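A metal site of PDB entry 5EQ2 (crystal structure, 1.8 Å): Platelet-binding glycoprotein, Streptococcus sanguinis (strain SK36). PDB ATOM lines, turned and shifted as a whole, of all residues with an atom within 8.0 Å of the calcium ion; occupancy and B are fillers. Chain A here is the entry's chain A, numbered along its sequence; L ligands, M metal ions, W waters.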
ATOM      1  N   ALA A 122     -32.850  21.975  12.322  1.00  0.00           N
ATOM      2  CA  ALA A 122     -32.228  20.657  12.489  1.00  0.00           C
ATOM      3  C   ALA A 122     -30.758  20.711  12.125  1.00  0.00           C
ATOM      4  O   ALA A 122     -30.327  21.476  11.259  1.00  0.00           O
ATOM      5  CB  ALA A 122     -32.972  19.647  11.629  1.00  0.00           C
ATOM      6  N   GLN A 123     -29.957  19.859  12.784  1.00  0.00           N
ATOM      7  CA  GLN A 123     -28.524  19.861  12.520  1.00  0.00           C
ATOM      8  C   GLN A 123     -28.223  19.506  11.071  1.00  0.00           C
ATOM      9  O   GLN A 123     -27.194  19.928  10.533  1.00  0.00           O
ATOM     10  CB  GLN A 123     -27.820  18.872  13.450  1.00  0.00           C
ATOM     11  CG  GLN A 123     -27.708  19.413  14.848  1.00  0.00           C
ATOM     12  CD  GLN A 123     -27.211  18.350  15.796  1.00  0.00           C
ATOM     13  OE1 GLN A 123     -27.871  17.339  16.000  1.00  0.00           O
ATOM     14  NE2 GLN A 123     -26.040  18.572  16.369  1.00  0.00           N
ATOM     15  N   THR A 124     -29.109  18.772  10.424  1.00  0.00           N
ATOM     16  CA  THR A 124     -28.835  18.431   9.031  1.00  0.00           C
ATOM     17  C   THR A 124     -28.874  19.666   8.152  1.00  0.00           C
ATOM     18  O   THR A 124     -28.332  19.633   7.041  1.00  0.00           O
ATOM     19  CB  THR A 124     -29.823  17.372   8.529  1.00  0.00           C
ATOM     20  OG1 THR A 124     -29.345  16.860   7.270  1.00  0.00           O
ATOM     21  CG2 THR A 124     -31.206  17.952   8.323  1.00  0.00           C
ATOM     22  N   ASP A 125     -29.464  20.760   8.628  1.00  0.00           N
ATOM     23  CA  ASP A 125     -29.421  21.998   7.856  1.00  0.00           C
ATOM     24  C   ASP A 125     -28.043  22.628   7.926  1.00  0.00           C
ATOM     25  O   ASP A 125     -27.652  23.359   7.011  1.00  0.00           O
ATOM     26  CB  ASP A 125     -30.496  22.962   8.361  1.00  0.00           C
ATOM     27  CG  ASP A 125     -31.898  22.510   7.998  1.00  0.00           C
ATOM     28  OD1 ASP A 125     -32.039  21.389   7.448  1.00  0.00           O
ATOM     29  OD2 ASP A 125     -32.875  23.265   8.271  1.00  0.00           O
ATOM     30  N   LYS A 126     -27.293  22.355   8.991  1.00  0.00           N
ATOM     31  CA  LYS A 126     -25.978  22.952   9.117  1.00  0.00           C
ATOM     32  C   LYS A 126     -24.911  22.177   8.361  1.00  0.00           C
ATOM     33  O   LYS A 126     -23.951  22.767   7.848  1.00  0.00           O
ATOM     34  CB  LYS A 126     -25.604  23.069  10.588  1.00  0.00           C
ATOM     35  CG  LYS A 126     -24.181  23.468  10.834  1.00  0.00           C
ATOM     36  CD  LYS A 126     -23.908  23.633  12.284  1.00  0.00           C
ATOM     37  CE  LYS A 126     -22.539  24.220  12.507  1.00  0.00           C
ATOM     38  NZ  LYS A 126     -22.045  23.904  13.872  1.00  0.00           N
ATOM     39  N   TYR A 127     -25.036  20.863   8.268  1.00  0.00           N
ATOM     40  CA  TYR A 127     -23.968  20.010   7.765  1.00  0.00           C
ATOM     41  C   TYR A 127     -24.279  19.524   6.361  1.00  0.00           C
ATOM     42  O   TYR A 127     -25.414  19.118   6.084  1.00  0.00           O
ATOM     43  CB  TYR A 127     -23.735  18.850   8.720  1.00  0.00           C
ATOM     44  CG  TYR A 127     -23.325  19.330  10.055  1.00  0.00           C
ATOM     45  CD1 TYR A 127     -22.059  19.851  10.255  1.00  0.00           C
ATOM     46  CD2 TYR A 127     -24.207  19.305  11.137  1.00  0.00           C
ATOM     47  CE1 TYR A 127     -21.672  20.309  11.498  1.00  0.00           C
ATOM     48  CE2 TYR A 127     -23.822  19.772  12.377  1.00  0.00           C
ATOM     49  CZ  TYR A 127     -22.562  20.279  12.549  1.00  0.00           C
ATOM     50  OH  TYR A 127     -22.156  20.746  13.770  1.00  0.00           O
ATOM     51  N   ASN A 128     -23.280  19.563   5.494  1.00  0.00           N
ATOM     52  CA  ASN A 128     -23.409  19.041   4.129  1.00  0.00           C
ATOM     53  C   ASN A 128     -22.286  18.041   3.912  1.00  0.00           C
ATOM     54  O   ASN A 128     -21.128  18.439   3.680  1.00  0.00           O
ATOM     55  CB  ASN A 128     -23.369  20.148   3.093  1.00  0.00           C
ATOM     56  CG  ASN A 128     -23.533  19.638   1.676  1.00  0.00           C
ATOM     57  OD1 ASN A 128     -22.628  19.731   0.852  1.00  0.00           O
ATOM     58  ND2 ASN A 128     -24.708  19.071   1.399  1.00  0.00           N
ATOM     59  N   PRO A 129     -22.565  16.733   3.988  1.00  0.00           N
ATOM     60  CA  PRO A 129     -21.472  15.748   3.943  1.00  0.00           C
ATOM     61  C   PRO A 129     -20.829  15.686   2.568  1.00  0.00           C
ATOM     62  O   PRO A 129     -21.504  15.649   1.540  1.00  0.00           O
ATOM     63  CB  PRO A 129     -22.166  14.429   4.307  1.00  0.00           C
ATOM     64  CG  PRO A 129     -23.593  14.628   3.953  1.00  0.00           C
ATOM     65  CD  PRO A 129     -23.873  16.095   4.199  1.00  0.00           C
ATOM     66  N   ILE A 162     -18.286  17.394  10.679  1.00  0.00           N
ATOM     67  CA  ILE A 162     -19.527  16.820  11.188  1.00  0.00           C
ATOM     68  C   ILE A 162     -19.281  16.423  12.643  1.00  0.00           C
ATOM     69  O   ILE A 162     -18.139  16.128  13.000  1.00  0.00           O
ATOM     70  CB  ILE A 162     -19.979  15.644  10.290  1.00  0.00           C
ATOM     71  CG1 ILE A 162     -20.858  16.141   9.158  1.00  0.00           C
ATOM     72  CG2 ILE A 162     -20.619  14.511  11.066  1.00  0.00           C
ATOM     73  CD1 ILE A 162     -21.328  15.108   8.238  1.00  0.00           C
ATOM     74  N   ILE A 178     -26.113   9.235   7.822  1.00  0.00           N
ATOM     75  CA  ILE A 178     -25.523  10.003   8.908  1.00  0.00           C
ATOM     76  C   ILE A 178     -26.668  10.508   9.761  1.00  0.00           C
ATOM     77  O   ILE A 178     -27.529  11.252   9.272  1.00  0.00           O
ATOM     78  CB  ILE A 178     -24.655  11.165   8.402  1.00  0.00           C
ATOM     79  CG1 ILE A 178     -23.549  10.652   7.481  1.00  0.00           C
ATOM     80  CG2 ILE A 178     -24.097  11.987   9.592  1.00  0.00           C
ATOM     81  CD1 ILE A 178     -22.859  11.732   6.699  1.00  0.00           C
ATOM     82  N   TYR A 180     -27.462  12.739  12.855  1.00  0.00           N
ATOM     83  CA  TYR A 180     -26.924  13.762  13.724  1.00  0.00           C
ATOM     84  C   TYR A 180     -27.473  13.611  15.136  1.00  0.00           C
ATOM     85  O   TYR A 180     -28.475  12.945  15.358  1.00  0.00           O
ATOM     86  CB  TYR A 180     -27.234  15.150  13.137  1.00  0.00           C
ATOM     87  CG  TYR A 180     -26.595  15.312  11.787  1.00  0.00           C
ATOM     88  CD1 TYR A 180     -25.236  15.550  11.663  1.00  0.00           C
ATOM     89  CD2 TYR A 180     -27.341  15.183  10.621  1.00  0.00           C
ATOM     90  CE1 TYR A 180     -24.640  15.677  10.428  1.00  0.00           C
ATOM     91  CE2 TYR A 180     -26.757  15.311   9.372  1.00  0.00           C
ATOM     92  CZ  TYR A 180     -25.403  15.563   9.285  1.00  0.00           C
ATOM     93  OH  TYR A 180     -24.794  15.684   8.053  1.00  0.00           O
ATOM     94  N   SER A 184     -31.929  14.187  13.166  1.00  0.00           N
ATOM     95  CA  SER A 184     -32.044  14.514  11.734  1.00  0.00           C
ATOM     96  C   SER A 184     -30.930  13.788  10.977  1.00  0.00           C
ATOM     97  O   SER A 184     -29.967  13.293  11.573  1.00  0.00           O
ATOM     98  CB  SER A 184     -31.983  16.033  11.496  1.00  0.00           C
ATOM     99  OG  SER A 184     -30.695  16.576  11.788  1.00  0.00           O
ATOM    100  N   THR A 185     -31.069  13.686   9.652  1.00  0.00           N
ATOM    101  CA  THR A 185     -30.190  12.781   8.926  1.00  0.00           C
ATOM    102  C   THR A 185     -29.691  13.375   7.615  1.00  0.00           C
ATOM    103  O   THR A 185     -30.182  14.396   7.112  1.00  0.00           O
ATOM    104  CB  THR A 185     -30.838  11.434   8.576  1.00  0.00           C
ATOM    105  OG1 THR A 185     -31.936  11.632   7.670  1.00  0.00           O
ATOM    106  CG2 THR A 185     -31.336  10.719   9.812  1.00  0.00           C
ATOM    107  N   ASP A 186     -28.742  12.656   7.036  1.00  0.00           N
ATOM    108  CA  ASP A 186     -28.229  12.845   5.691  1.00  0.00           C
ATOM    109  C   ASP A 186     -27.942  11.469   5.133  1.00  0.00           C
ATOM    110  O   ASP A 186     -27.616  10.541   5.890  1.00  0.00           O
ATOM    111  CB  ASP A 186     -26.983  13.738   5.711  1.00  0.00           C
ATOM    112  CG  ASP A 186     -27.334  15.188   5.589  1.00  0.00           C
ATOM    113  OD1 ASP A 186     -26.551  16.048   6.048  1.00  0.00           O
ATOM    114  OD2 ASP A 186     -28.369  15.432   4.965  1.00  0.00           O
ATOM    115  N   THR A 187     -28.126  11.312   3.822  1.00  0.00           N
ATOM    116  CA  THR A 187     -27.896  10.049   3.119  1.00  0.00           C
ATOM    117  C   THR A 187     -26.845  10.257   2.039  1.00  0.00           C
ATOM    118  O   THR A 187     -26.778  11.321   1.430  1.00  0.00           O
ATOM    119  CB  THR A 187     -29.183   9.495   2.467  1.00  0.00           C
ATOM    120  OG1 THR A 187     -30.206   9.363   3.460  1.00  0.00           O
ATOM    121  CG2 THR A 187     -28.935   8.112   1.842  1.00  0.00           C
HETATM  122  C1  LIG L   1     -29.881  18.087   4.455  1.00  0.00           C
HETATM  123  O1  LIG L   1     -29.006  17.595   5.188  1.00  0.00           O
HETATM  124  O2  LIG L   1     -29.522  19.077   3.786  1.00  0.00           O
HETATM  125  C2  LIG L   1     -31.275  17.529   4.410  1.00  0.00           C
HETATM  126 CA    CA M   1     -27.236  18.274   5.469  1.00  0.00          CA
HETATM  127  O   HOH W   1     -27.004  20.721   4.451  1.00  0.00           O
HETATM  128  O   HOH W   2     -26.327  17.796   3.274  1.00  0.00           O
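OH of Tyr 127 sits at hydrogen-bond distance from NZ of Lys 126 (3.2 Å).
The side-chain hydroxyl (OG1) of Thr 124 is in hydrogen-bond range of the backbone carbonyl oxygen (O) of Thr 185 (2.6 Å).
The backbone NH of Thr 124 lies within hydrogen-bond range of the side-chain hydroxyl of Ser 184 (3.0 Å).
The side-chain hydroxyl (OH) of Tyr 180 sits close to the side-chain carboxylate (OD1) of Asp 186, 2.7 Å away.
O of Asp 186 lies within hydrogen-bond range of N of Ile 178, 2.8 Å away.
Within 4 Å of the calcium ion: Thr 124, Tyr 127 and Asp 186.
Along chain A the residues within 4 Å of the calcium ion span positions 124 to 186.
O1 of the ligand is bound to the calcium ion (1.9 Å).
The calcium ion is bound by the backbone carbonyl oxygen (O) of Tyr 127 (2.1 Å).
The calcium ion is bound by O of Thr 124.
OD1 of Asp 186 is bound to the calcium ion (2.4 Å).
Water W2 binds the calcium ion (2.4 Å).
Water W1 is bound to the calcium ion.
Slightly farther from the calcium ion lies an oxygen (O2) of the ligand (3.0 Å).
Slightly farther from the calcium ion lies OD2 of Asp 186 (3.1 Å).
Slightly farther from the calcium ion lies the side-chain hydroxyl (OG1) of Thr 124 (3.1 Å).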
